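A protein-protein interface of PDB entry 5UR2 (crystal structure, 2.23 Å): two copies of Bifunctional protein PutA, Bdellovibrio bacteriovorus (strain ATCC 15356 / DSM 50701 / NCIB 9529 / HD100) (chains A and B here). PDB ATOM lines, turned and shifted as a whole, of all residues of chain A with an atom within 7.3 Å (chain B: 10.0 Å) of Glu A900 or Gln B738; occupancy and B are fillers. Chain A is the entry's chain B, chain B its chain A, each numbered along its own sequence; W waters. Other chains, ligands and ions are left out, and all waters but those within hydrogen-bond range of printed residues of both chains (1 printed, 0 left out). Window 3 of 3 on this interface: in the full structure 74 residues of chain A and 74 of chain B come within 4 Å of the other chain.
No position is printed for both chains. Of the 9 pairs that touch across the chains among the printed residues, none has its exchanged pair printed and touching as well.
NE of Arg B632 is in salt-bridge range of OE2 of Glu B966, at 2.8 Å. The backbone carbonyl oxygen (O) of Thr B711 lies within hydrogen-bond range of a ring nitrogen (NE2) of His B739. NZ of Lys A947 lies within hydrogen-bond range of O of Asn A897 (3.1 Å). The backbone carbonyl oxygen (O) of Glu A900 sits at hydrogen-bond distance from the backbone NH (N) of Met A948, at 3.0 Å. The backbone NH (N) of Phe A946 lies within hydrogen-bond range of the backbone carbonyl oxygen (O) of Ala A902 (3.1 Å). NZ of Lys A720 lies within salt-bridge range of OE2 of Glu A900 (2.8 Å).
Water W1 bridges O of Lys A947 (2.6 Å) and N of Val B740 (2.8 Å).
Of the printed residues of chain B, Glu A900 touches Gln B738 (3.99 Å). Printed residues of chain A within 4 Å of Gln B738: Thr A899, Glu A900, Lys A947 and Met A948. Printed residues of chain B within 4 Å of Met A948: Gln B738 and His B739. Of the printed residues of chain B, Leu A724 touches Val B733. Of the printed residues of chain A, Val B740 touches Lys A947. Printed residues of chain A within 4 Å of Val B733: Leu A724. The nearest printed residue of chain A that does not touch Gln B738 is Ser A898 (5.2 Å). The nearest printed residue of chain B that does not touch Leu A724 is Val B740 (4.9 Å).
N of His B739 is in hydrogen-bond range of SD of Met A948 (3.5 Å).
CG2 of Val B733 touches CD2 of Leu A724, 3.95 Å away. Gln B738 touches Thr A899 (OE1 to O, 3.7 Å). Glu A900 touches Gln B738 (CG to NE2, 3.99 Å). Phe A946 touches Glu B966 (CB to OE1, 3.8 Å). Lys A947 touches Gln B738 (CB to O, 3.3 Å). Lys A947 touches His B739. Lys A947 touches Val B740. Gln B738 touches Met A948.
Of the 18 printed residues of chain B, 5 touch a printed residue of chain A. Hydrophobic or aromatic side chains of chain A that line the printed part of chain B: Leu A724, Phe A946 and Met A948.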
ATOM      1  N   LYS A 720      -7.324  -3.543  -8.424  1.00  0.00           N
ATOM      2  CA  LYS A 720      -7.782  -2.260  -7.912  1.00  0.00           C
ATOM      3  C   LYS A 720      -8.679  -2.457  -6.695  1.00  0.00           C
ATOM      4  O   LYS A 720      -8.529  -1.765  -5.682  1.00  0.00           O
ATOM      5  CB  LYS A 720      -8.535  -1.508  -9.006  1.00  0.00           C
ATOM      6  CG  LYS A 720      -8.790  -0.043  -8.697  1.00  0.00           C
ATOM      7  CD  LYS A 720      -9.697   0.596  -9.748  1.00  0.00           C
ATOM      8  CE  LYS A 720     -11.105   0.030  -9.623  1.00  0.00           C
ATOM      9  NZ  LYS A 720     -12.110   0.844 -10.313  1.00  0.00           N
ATOM     10  N   LEU A 724      -7.767  -0.699  -3.122  1.00  0.00           N
ATOM     11  CA  LEU A 724      -8.598   0.285  -2.450  1.00  0.00           C
ATOM     12  C   LEU A 724      -9.002  -0.198  -1.063  1.00  0.00           C
ATOM     13  O   LEU A 724      -9.005   0.586  -0.106  1.00  0.00           O
ATOM     14  CB  LEU A 724      -9.837   0.602  -3.296  1.00  0.00           C
ATOM     15  CG  LEU A 724      -9.489   1.168  -4.678  1.00  0.00           C
ATOM     16  CD1 LEU A 724     -10.729   1.611  -5.420  1.00  0.00           C
ATOM     17  CD2 LEU A 724      -8.460   2.290  -4.603  1.00  0.00           C
ATOM     18  N   GLY A 748      -2.714  -2.166 -11.552  1.00  0.00           N
ATOM     19  CA  GLY A 748      -3.133  -2.554 -12.888  1.00  0.00           C
ATOM     20  C   GLY A 748      -3.382  -1.384 -13.826  1.00  0.00           C
ATOM     21  O   GLY A 748      -3.266  -0.204 -13.475  1.00  0.00           O
ATOM     22  N   GLY A 749      -3.740  -1.746 -15.062  1.00  0.00           N
ATOM     23  CA  GLY A 749      -3.903  -0.769 -16.119  1.00  0.00           C
ATOM     24  C   GLY A 749      -4.860  -1.245 -17.187  1.00  0.00           C
ATOM     25  O   GLY A 749      -5.344  -2.379 -17.170  1.00  0.00           O
ATOM     26  N   LYS A 750      -5.169  -0.319 -18.097  1.00  0.00           N
ATOM     27  CA  LYS A 750      -5.907  -0.578 -19.332  1.00  0.00           C
ATOM     28  C   LYS A 750      -5.068   0.082 -20.418  1.00  0.00           C
ATOM     29  O   LYS A 750      -5.369   1.189 -20.864  1.00  0.00           O
ATOM     30  CB  LYS A 750      -7.328  -0.016 -19.282  1.00  0.00           C
ATOM     31  CG  LYS A 750      -8.202  -0.421 -20.451  1.00  0.00           C
ATOM     32  CD  LYS A 750      -8.540  -1.903 -20.400  1.00  0.00           C
ATOM     33  CE  LYS A 750      -9.325  -2.365 -21.628  1.00  0.00           C
ATOM     34  NZ  LYS A 750      -9.692  -3.817 -21.526  1.00  0.00           N
ATOM     35  N   GLN A 873     -12.428  -0.255 -21.258  1.00  0.00           N
ATOM     36  CA  GLN A 873     -12.279   0.465 -19.988  1.00  0.00           C
ATOM     37  C   GLN A 873     -11.919  -0.444 -18.813  1.00  0.00           C
ATOM     38  O   GLN A 873     -11.067  -0.074 -17.998  1.00  0.00           O
ATOM     39  CB  GLN A 873     -13.584   1.259 -19.653  1.00  0.00           C
ATOM     40  CG  GLN A 873     -13.860   2.480 -20.548  1.00  0.00           C
ATOM     41  CD  GLN A 873     -12.885   3.640 -20.286  1.00  0.00           C
ATOM     42  OE1 GLN A 873     -12.410   3.835 -19.162  1.00  0.00           O
ATOM     43  NE2 GLN A 873     -12.562   4.389 -21.336  1.00  0.00           N
ATOM     44  N   ALA A 874     -12.562  -1.605 -18.686  1.00  0.00           N
ATOM     45  CA  ALA A 874     -12.327  -2.505 -17.562  1.00  0.00           C
ATOM     46  C   ALA A 874     -11.157  -3.428 -17.862  1.00  0.00           C
ATOM     47  O   ALA A 874     -11.057  -3.985 -18.960  1.00  0.00           O
ATOM     48  CB  ALA A 874     -13.584  -3.335 -17.265  1.00  0.00           C
ATOM     49  N   GLU A 875     -10.265  -3.590 -16.883  1.00  0.00           N
ATOM     50  CA  GLU A 875      -9.100  -4.452 -17.077  1.00  0.00           C
ATOM     51  C   GLU A 875      -9.540  -5.907 -17.084  1.00  0.00           C
ATOM     52  O   GLU A 875     -10.323  -6.328 -16.229  1.00  0.00           O
ATOM     53  CB  GLU A 875      -8.051  -4.224 -15.984  1.00  0.00           C
ATOM     54  CG  GLU A 875      -6.778  -5.070 -16.159  1.00  0.00           C
ATOM     55  CD  GLU A 875      -5.768  -4.871 -15.023  1.00  0.00           C
ATOM     56  OE1 GLU A 875      -6.208  -4.851 -13.851  1.00  0.00           O
ATOM     57  OE2 GLU A 875      -4.540  -4.764 -15.295  1.00  0.00           O
ATOM     58  N   ASN A 897      -6.214   8.487 -23.091  1.00  0.00           N
ATOM     59  CA  ASN A 897      -6.247   9.109 -21.775  1.00  0.00           C
ATOM     60  C   ASN A 897      -7.581   8.943 -21.048  1.00  0.00           C
ATOM     61  O   ASN A 897      -7.721   9.449 -19.934  1.00  0.00           O
ATOM     62  CB  ASN A 897      -5.928  10.601 -21.909  1.00  0.00           C
ATOM     63  CG  ASN A 897      -4.466  10.857 -22.179  1.00  0.00           C
ATOM     64  OD1 ASN A 897      -3.587  10.105 -21.736  1.00  0.00           O
ATOM     65  ND2 ASN A 897      -4.191  11.912 -22.928  1.00  0.00           N
ATOM     66  N   SER A 898      -8.544   8.231 -21.626  1.00  0.00           N
ATOM     67  CA  SER A 898      -9.919   8.253 -21.158  1.00  0.00           C
ATOM     68  C   SER A 898     -10.246   7.177 -20.124  1.00  0.00           C
ATOM     69  O   SER A 898     -11.416   7.032 -19.773  1.00  0.00           O
ATOM     70  CB  SER A 898     -10.862   8.111 -22.362  1.00  0.00           C
ATOM     71  OG  SER A 898     -10.780   6.792 -22.921  1.00  0.00           O
ATOM     72  N   THR A 899      -9.263   6.431 -19.616  1.00  0.00           N
ATOM     73  CA  THR A 899      -9.552   5.360 -18.673  1.00  0.00           C
ATOM     74  C   THR A 899      -9.278   5.797 -17.232  1.00  0.00           C
ATOM     75  O   THR A 899      -8.815   6.904 -16.951  1.00  0.00           O
ATOM     76  CB  THR A 899      -8.751   4.075 -18.970  1.00  0.00           C
ATOM     77  OG1 THR A 899      -7.404   4.205 -18.491  1.00  0.00           O
ATOM     78  CG2 THR A 899      -8.720   3.740 -20.459  1.00  0.00           C
ATOM     79  N   GLU A 900      -9.582   4.875 -16.313  1.00  0.00           N
ATOM     80  CA  GLU A 900      -9.257   4.979 -14.900  1.00  0.00           C
ATOM     81  C   GLU A 900      -7.766   4.853 -14.622  1.00  0.00           C
ATOM     82  O   GLU A 900      -7.323   5.206 -13.528  1.00  0.00           O
ATOM     83  CB  GLU A 900      -9.974   3.851 -14.148  1.00  0.00           C
ATOM     84  CG  GLU A 900     -11.207   4.224 -13.367  1.00  0.00           C
ATOM     85  CD  GLU A 900     -11.746   3.034 -12.569  1.00  0.00           C
ATOM     86  OE1 GLU A 900     -11.360   1.875 -12.852  1.00  0.00           O
ATOM     87  OE2 GLU A 900     -12.543   3.264 -11.637  1.00  0.00           O
ATOM     88  N   TYR A 901      -6.990   4.369 -15.581  1.00  0.00           N
ATOM     89  CA  TYR A 901      -5.651   3.872 -15.337  1.00  0.00           C
ATOM     90  C   TYR A 901      -4.601   4.720 -16.041  1.00  0.00           C
ATOM     91  O   TYR A 901      -4.889   5.458 -16.989  1.00  0.00           O
ATOM     92  CB  TYR A 901      -5.537   2.411 -15.794  1.00  0.00           C
ATOM     93  CG  TYR A 901      -6.433   1.465 -15.018  1.00  0.00           C
ATOM     94  CD1 TYR A 901      -6.109   1.091 -13.711  1.00  0.00           C
ATOM     95  CD2 TYR A 901      -7.585   0.925 -15.591  1.00  0.00           C
ATOM     96  CE1 TYR A 901      -6.911   0.221 -12.998  1.00  0.00           C
ATOM     97  CE2 TYR A 901      -8.401   0.052 -14.878  1.00  0.00           C
ATOM     98  CZ  TYR A 901      -8.064  -0.293 -13.584  1.00  0.00           C
ATOM     99  OH  TYR A 901      -8.858  -1.166 -12.873  1.00  0.00           O
ATOM    100  N   ALA A 902      -3.370   4.606 -15.556  1.00  0.00           N
ATOM    101  CA  ALA A 902      -2.260   5.375 -16.100  1.00  0.00           C
ATOM    102  C   ALA A 902      -0.957   4.625 -15.827  1.00  0.00           C
ATOM    103  O   ALA A 902      -0.010   5.146 -15.224  1.00  0.00           O
ATOM    104  CB  ALA A 902      -2.260   6.780 -15.501  1.00  0.00           C
ATOM    105  N   LEU A 903      -0.894   3.369 -16.278  1.00  0.00           N
ATOM    106  CA  LEU A 903       0.271   2.531 -16.031  1.00  0.00           C
ATOM    107  C   LEU A 903       1.206   2.548 -17.247  1.00  0.00           C
ATOM    108  O   LEU A 903       2.169   3.324 -17.246  1.00  0.00           O
ATOM    109  CB  LEU A 903      -0.175   1.113 -15.652  1.00  0.00           C
ATOM    110  CG  LEU A 903       0.921   0.137 -15.188  1.00  0.00           C
ATOM    111  CD1 LEU A 903       1.940   0.817 -14.301  1.00  0.00           C
ATOM    112  CD2 LEU A 903       0.315  -1.068 -14.486  1.00  0.00           C
ATOM    113  N   PHE A 946       0.122   6.028 -12.228  1.00  0.00           N
ATOM    114  CA  PHE A 946      -0.720   6.851 -11.378  1.00  0.00           C
ATOM    115  C   PHE A 946      -2.189   6.663 -11.747  1.00  0.00           C
ATOM    116  O   PHE A 946      -2.558   5.600 -12.256  1.00  0.00           O
ATOM    117  CB  PHE A 946      -0.270   8.331 -11.445  1.00  0.00           C
ATOM    118  CG  PHE A 946       0.105   8.828 -12.838  1.00  0.00           C
ATOM    119  CD1 PHE A 946       1.380   8.603 -13.351  1.00  0.00           C
ATOM    120  CD2 PHE A 946      -0.797   9.578 -13.595  1.00  0.00           C
ATOM    121  CE1 PHE A 946       1.745   9.068 -14.622  1.00  0.00           C
ATOM    122  CE2 PHE A 946      -0.446  10.048 -14.876  1.00  0.00           C
ATOM    123  CZ  PHE A 946       0.841   9.794 -15.384  1.00  0.00           C
ATOM    124  N   LYS A 947      -3.027   7.678 -11.492  1.00  0.00           N
ATOM    125  CA  LYS A 947      -4.475   7.500 -11.473  1.00  0.00           C
ATOM    126  C   LYS A 947      -4.751   6.261 -10.628  1.00  0.00           C
ATOM    127  O   LYS A 947      -4.101   6.084  -9.592  1.00  0.00           O
ATOM    128  CB  LYS A 947      -5.042   7.386 -12.888  1.00  0.00           C
ATOM    129  CG  LYS A 947      -4.939   8.684 -13.715  1.00  0.00           C
ATOM    130  CD  LYS A 947      -5.719   8.582 -15.039  1.00  0.00           C
ATOM    131  CE  LYS A 947      -5.457   9.789 -15.947  1.00  0.00           C
ATOM    132  NZ  LYS A 947      -6.112   9.726 -17.323  1.00  0.00           N
ATOM    133  N   MET A 948      -5.627   5.358 -11.081  1.00  0.00           N
ATOM    134  CA  MET A 948      -5.949   4.163 -10.299  1.00  0.00           C
ATOM    135  C   MET A 948      -4.958   3.001 -10.508  1.00  0.00           C
ATOM    136  O   MET A 948      -5.240   1.882 -10.061  1.00  0.00           O
ATOM    137  CB  MET A 948      -7.384   3.698 -10.592  1.00  0.00           C
ATOM    138  CG  MET A 948      -8.477   4.715 -10.206  1.00  0.00           C
ATOM    139  SD  MET A 948      -8.366   5.306  -8.486  1.00  0.00           S
ATOM    140  CE  MET A 948      -8.693   3.779  -7.645  1.00  0.00           C
ATOM    141  N   SER A 949      -3.799   3.241 -11.127  1.00  0.00           N
ATOM    142  CA  SER A 949      -2.775   2.211 -11.277  1.00  0.00           C
ATOM    143  C   SER A 949      -1.859   2.075 -10.066  1.00  0.00           C
ATOM    144  O   SER A 949      -1.080   1.119 -10.013  1.00  0.00           O
ATOM    145  CB  SER A 949      -1.913   2.474 -12.520  1.00  0.00           C
ATOM    146  OG  SER A 949      -2.702   2.358 -13.685  1.00  0.00           O
ATOM    147  N   GLN B 543      -8.722  23.428 -10.636  1.00  0.00           N
ATOM    148  CA  GLN B 543      -8.704  22.372 -11.641  1.00  0.00           C
ATOM    149  C   GLN B 543      -8.604  22.958 -13.047  1.00  0.00           C
ATOM    150  O   GLN B 543      -7.809  22.483 -13.871  1.00  0.00           O
ATOM    151  CB  GLN B 543      -9.948  21.487 -11.471  1.00  0.00           C
ATOM    152  CG  GLN B 543     -10.039  20.308 -12.417  1.00  0.00           C
ATOM    153  CD  GLN B 543      -8.916  19.295 -12.218  1.00  0.00           C
ATOM    154  OE1 GLN B 543      -8.346  19.164 -11.127  1.00  0.00           O
ATOM    155  NE2 GLN B 543      -8.579  18.589 -13.287  1.00  0.00           N
ATOM    156  N   ARG B 632       0.876  16.390 -10.050  1.00  0.00           N
ATOM    157  CA  ARG B 632      -0.262  15.542  -9.682  1.00  0.00           C
ATOM    158  C   ARG B 632      -1.624  16.172  -9.929  1.00  0.00           C
ATOM    159  O   ARG B 632      -2.530  15.480 -10.378  1.00  0.00           O
ATOM    160  CB  ARG B 632      -0.199  15.135  -8.193  1.00  0.00           C
ATOM    161  CG  ARG B 632       1.101  14.469  -7.772  1.00  0.00           C
ATOM    162  CD  ARG B 632       1.016  13.746  -6.409  1.00  0.00           C
ATOM    163  NE  ARG B 632       0.384  12.448  -6.559  1.00  0.00           N
ATOM    164  CZ  ARG B 632      -0.767  12.090  -6.014  1.00  0.00           C
ATOM    165  NH1 ARG B 632      -1.434  12.931  -5.234  1.00  0.00           N
ATOM    166  NH2 ARG B 632      -1.238  10.870  -6.234  1.00  0.00           N
ATOM    167  N   HIS B 708     -12.997  16.472  -1.729  1.00  0.00           N
ATOM    168  CA  HIS B 708     -13.376  16.736  -3.113  1.00  0.00           C
ATOM    169  C   HIS B 708     -12.705  15.758  -4.086  1.00  0.00           C
ATOM    170  O   HIS B 708     -11.581  15.303  -3.871  1.00  0.00           O
ATOM    171  CB  HIS B 708     -13.022  18.180  -3.476  1.00  0.00           C
ATOM    172  CG  HIS B 708     -13.751  18.691  -4.674  1.00  0.00           C
ATOM    173  ND1 HIS B 708     -13.342  18.417  -5.963  1.00  0.00           N
ATOM    174  CD2 HIS B 708     -14.884  19.428  -4.784  1.00  0.00           C
ATOM    175  CE1 HIS B 708     -14.181  18.982  -6.815  1.00  0.00           C
ATOM    176  NE2 HIS B 708     -15.130  19.595  -6.126  1.00  0.00           N
ATOM    177  N   LYS B 709     -13.403  15.451  -5.184  1.00  0.00           N
ATOM    178  CA  LYS B 709     -12.895  14.459  -6.131  1.00  0.00           C
ATOM    179  C   LYS B 709     -11.691  14.957  -6.917  1.00  0.00           C
ATOM    180  O   LYS B 709     -10.939  14.129  -7.440  1.00  0.00           O
ATOM    181  CB  LYS B 709     -14.002  14.008  -7.103  1.00  0.00           C
ATOM    182  CG  LYS B 709     -14.468  15.100  -8.041  1.00  0.00           C
ATOM    183  CD  LYS B 709     -15.623  14.675  -8.935  1.00  0.00           C
ATOM    184  CE  LYS B 709     -15.996  15.836  -9.854  1.00  0.00           C
ATOM    185  NZ  LYS B 709     -17.301  15.671 -10.554  1.00  0.00           N
ATOM    186  N   TYR B 710     -11.496  16.279  -7.028  1.00  0.00           N
ATOM    187  CA  TYR B 710     -10.350  16.825  -7.755  1.00  0.00           C
ATOM    188  C   TYR B 710      -9.087  16.887  -6.912  1.00  0.00           C
ATOM    189  O   TYR B 710      -7.988  17.018  -7.470  1.00  0.00           O
ATOM    190  CB  TYR B 710     -10.632  18.239  -8.267  1.00  0.00           C
ATOM    191  CG  TYR B 710     -11.657  18.347  -9.359  1.00  0.00           C
ATOM    192  CD1 TYR B 710     -12.018  17.254 -10.121  1.00  0.00           C
ATOM    193  CD2 TYR B 710     -12.297  19.554  -9.596  1.00  0.00           C
ATOM    194  CE1 TYR B 710     -12.985  17.362 -11.117  1.00  0.00           C
ATOM    195  CE2 TYR B 710     -13.249  19.679 -10.576  1.00  0.00           C
ATOM    196  CZ  TYR B 710     -13.596  18.584 -11.338  1.00  0.00           C
ATOM    197  OH  TYR B 710     -14.556  18.734 -12.311  1.00  0.00           O
ATOM    198  N   THR B 711      -9.203  16.826  -5.592  1.00  0.00           N
ATOM    199  CA  THR B 711      -8.020  16.972  -4.755  1.00  0.00           C
ATOM    200  C   THR B 711      -7.117  15.752  -4.912  1.00  0.00           C
ATOM    201  O   THR B 711      -7.537  14.623  -4.647  1.00  0.00           O
ATOM    202  CB  THR B 711      -8.426  17.164  -3.299  1.00  0.00           C
ATOM    203  OG1 THR B 711      -9.216  18.360  -3.179  1.00  0.00           O
ATOM    204  CG2 THR B 711      -7.180  17.237  -2.393  1.00  0.00           C
ATOM    205  N   THR B 712      -5.891  15.967  -5.379  1.00  0.00           N
ATOM    206  CA  THR B 712      -4.940  14.871  -5.520  1.00  0.00           C
ATOM    207  C   THR B 712      -3.991  14.760  -4.337  1.00  0.00           C
ATOM    208  O   THR B 712      -3.566  13.656  -3.994  1.00  0.00           O
ATOM    209  CB  THR B 712      -4.110  15.034  -6.800  1.00  0.00           C
ATOM    210  OG1 THR B 712      -3.431  16.290  -6.762  1.00  0.00           O
ATOM    211  CG2 THR B 712      -4.996  14.985  -8.036  1.00  0.00           C
ATOM    212  N   VAL B 732     -10.876   7.557   1.176  1.00  0.00           N
ATOM    213  CA  VAL B 732     -12.127   7.338   0.455  1.00  0.00           C
ATOM    214  C   VAL B 732     -11.969   7.783  -0.995  1.00  0.00           C
ATOM    215  O   VAL B 732     -11.543   8.911  -1.274  1.00  0.00           O
ATOM    216  CB  VAL B 732     -13.278   8.093   1.137  1.00  0.00           C
ATOM    217  CG1 VAL B 732     -14.576   7.940   0.341  1.00  0.00           C
ATOM    218  CG2 VAL B 732     -13.445   7.599   2.574  1.00  0.00           C
ATOM    219  N   VAL B 733     -12.343   6.904  -1.918  1.00  0.00           N
ATOM    220  CA  VAL B 733     -12.380   7.224  -3.339  1.00  0.00           C
ATOM    221  C   VAL B 733     -13.770   7.761  -3.643  1.00  0.00           C
ATOM    222  O   VAL B 733     -14.744   7.005  -3.684  1.00  0.00           O
ATOM    223  CB  VAL B 733     -12.048   6.005  -4.207  1.00  0.00           C
ATOM    224  CG1 VAL B 733     -12.144   6.367  -5.690  1.00  0.00           C
ATOM    225  CG2 VAL B 733     -10.643   5.500  -3.872  1.00  0.00           C
ATOM    226  N   GLN B 734     -13.857   9.070  -3.864  1.00  0.00           N
ATOM    227  CA  GLN B 734     -15.130   9.709  -4.086  1.00  0.00           C
ATOM    228  C   GLN B 734     -15.700   9.291  -5.436  1.00  0.00           C
ATOM    229  O   GLN B 734     -14.957   8.909  -6.342  1.00  0.00           O
ATOM    230  CB  GLN B 734     -14.959  11.224  -4.039  1.00  0.00           C
ATOM    231  CG  GLN B 734     -14.400  11.736  -2.716  1.00  0.00           C
ATOM    232  CD  GLN B 734     -15.391  11.585  -1.558  1.00  0.00           C
ATOM    233  OE1 GLN B 734     -16.602  11.525  -1.776  1.00  0.00           O
ATOM    234  NE2 GLN B 734     -14.877  11.542  -0.321  1.00  0.00           N
ATOM    235  N   PRO B 735     -17.020   9.373  -5.601  1.00  0.00           N
ATOM    236  CA  PRO B 735     -17.603   9.172  -6.933  1.00  0.00           C
ATOM    237  C   PRO B 735     -16.943  10.091  -7.951  1.00  0.00           C
ATOM    238  O   PRO B 735     -16.774  11.293  -7.718  1.00  0.00           O
ATOM    239  CB  PRO B 735     -19.082   9.516  -6.724  1.00  0.00           C
ATOM    240  CG  PRO B 735     -19.326   9.194  -5.292  1.00  0.00           C
ATOM    241  CD  PRO B 735     -18.052   9.526  -4.560  1.00  0.00           C
ATOM    242  N   GLY B 736     -16.526   9.507  -9.073  1.00  0.00           N
ATOM    243  CA  GLY B 736     -15.855  10.256 -10.118  1.00  0.00           C
ATOM    244  C   GLY B 736     -14.386  10.550  -9.876  1.00  0.00           C
ATOM    245  O   GLY B 736     -13.736  11.120 -10.759  1.00  0.00           O
ATOM    246  N   GLN B 737     -13.837  10.164  -8.728  1.00  0.00           N
ATOM    247  CA  GLN B 737     -12.422  10.355  -8.442  1.00  0.00           C
ATOM    248  C   GLN B 737     -11.630   9.238  -9.115  1.00  0.00           C
ATOM    249  O   GLN B 737     -11.901   8.059  -8.882  1.00  0.00           O
ATOM    250  CB  GLN B 737     -12.191  10.346  -6.935  1.00  0.00           C
ATOM    251  CG  GLN B 737     -10.743  10.554  -6.491  1.00  0.00           C
ATOM    252  CD  GLN B 737     -10.573  10.297  -5.002  1.00  0.00           C
ATOM    253  OE1 GLN B 737     -11.442  10.663  -4.198  1.00  0.00           O
ATOM    254  NE2 GLN B 737      -9.461   9.643  -4.625  1.00  0.00           N
ATOM    255  N   GLN B 738     -10.657   9.601  -9.953  1.00  0.00           N
ATOM    256  CA  GLN B 738      -9.875   8.582 -10.647  1.00  0.00           C
ATOM    257  C   GLN B 738      -8.394   8.686 -10.297  1.00  0.00           C
ATOM    258  O   GLN B 738      -7.537   8.683 -11.181  1.00  0.00           O
ATOM    259  CB  GLN B 738     -10.054   8.719 -12.152  1.00  0.00           C
ATOM    260  CG  GLN B 738     -11.474   8.566 -12.654  1.00  0.00           C
ATOM    261  CD  GLN B 738     -11.497   8.535 -14.150  1.00  0.00           C
ATOM    262  OE1 GLN B 738     -10.688   9.209 -14.790  1.00  0.00           O
ATOM    263  NE2 GLN B 738     -12.417   7.771 -14.728  1.00  0.00           N
ATOM    264  N   HIS B 739      -8.086   8.773  -9.016  1.00  0.00           N
ATOM    265  CA  HIS B 739      -6.705   8.812  -8.567  1.00  0.00           C
ATOM    266  C   HIS B 739      -6.722   8.466  -7.088  1.00  0.00           C
ATOM    267  O   HIS B 739      -7.781   8.372  -6.463  1.00  0.00           O
ATOM    268  CB  HIS B 739      -6.074  10.179  -8.801  1.00  0.00           C
ATOM    269  CG  HIS B 739      -6.771  11.267  -8.047  1.00  0.00           C
ATOM    270  ND1 HIS B 739      -7.752  12.053  -8.610  1.00  0.00           N
ATOM    271  CD2 HIS B 739      -6.678  11.652  -6.749  1.00  0.00           C
ATOM    272  CE1 HIS B 739      -8.201  12.903  -7.702  1.00  0.00           C
ATOM    273  NE2 HIS B 739      -7.568  12.676  -6.564  1.00  0.00           N
ATOM    274  N   VAL B 740      -5.540   8.235  -6.551  1.00  0.00           N
ATOM    275  CA  VAL B 740      -5.360   7.998  -5.134  1.00  0.00           C
ATOM    276  C   VAL B 740      -4.840   9.274  -4.494  1.00  0.00           C
ATOM    277  O   VAL B 740      -3.872   9.879  -4.972  1.00  0.00           O
ATOM    278  CB  VAL B 740      -4.408   6.815  -4.900  1.00  0.00           C
ATOM    279  CG1 VAL B 740      -4.261   6.553  -3.420  1.00  0.00           C
ATOM    280  CG2 VAL B 740      -4.962   5.583  -5.614  1.00  0.00           C
ATOM    281  N   LYS B 741      -5.480   9.687  -3.417  1.00  0.00           N
ATOM    282  CA  LYS B 741      -5.058  10.884  -2.726  1.00  0.00           C
ATOM    283  C   LYS B 741      -3.811  10.594  -1.904  1.00  0.00           C
ATOM    284  O   LYS B 741      -3.656   9.506  -1.343  1.00  0.00           O
ATOM    285  CB  LYS B 741      -6.191  11.396  -1.846  1.00  0.00           C
ATOM    286  CG  LYS B 741      -7.272  12.084  -2.636  1.00  0.00           C
ATOM    287  CD  LYS B 741      -8.461  12.421  -1.756  1.00  0.00           C
ATOM    288  CE  LYS B 741      -9.615  13.015  -2.566  1.00  0.00           C
ATOM    289  NZ  LYS B 741     -10.845  13.250  -1.719  1.00  0.00           N
ATOM    290  N   GLU B 966       4.694  12.879  -9.334  1.00  0.00           N
ATOM    291  CA  GLU B 966       4.714  11.464  -9.719  1.00  0.00           C
ATOM    292  C   GLU B 966       5.968  11.203 -10.531  1.00  0.00           C
ATOM    293  O   GLU B 966       6.264  11.981 -11.448  1.00  0.00           O
ATOM    294  CB  GLU B 966       3.484  11.078 -10.581  1.00  0.00           C
ATOM    295  CG  GLU B 966       2.152  11.039  -9.889  1.00  0.00           C
ATOM    296  CD  GLU B 966       2.037   9.921  -8.880  1.00  0.00           C
ATOM    297  OE1 GLU B 966       2.626   8.834  -9.100  1.00  0.00           O
ATOM    298  OE2 GLU B 966       1.333  10.124  -7.871  1.00  0.00           O
HETATM  299  O   HOH W   1      -3.225   8.048  -8.195  1.00  0.00           O
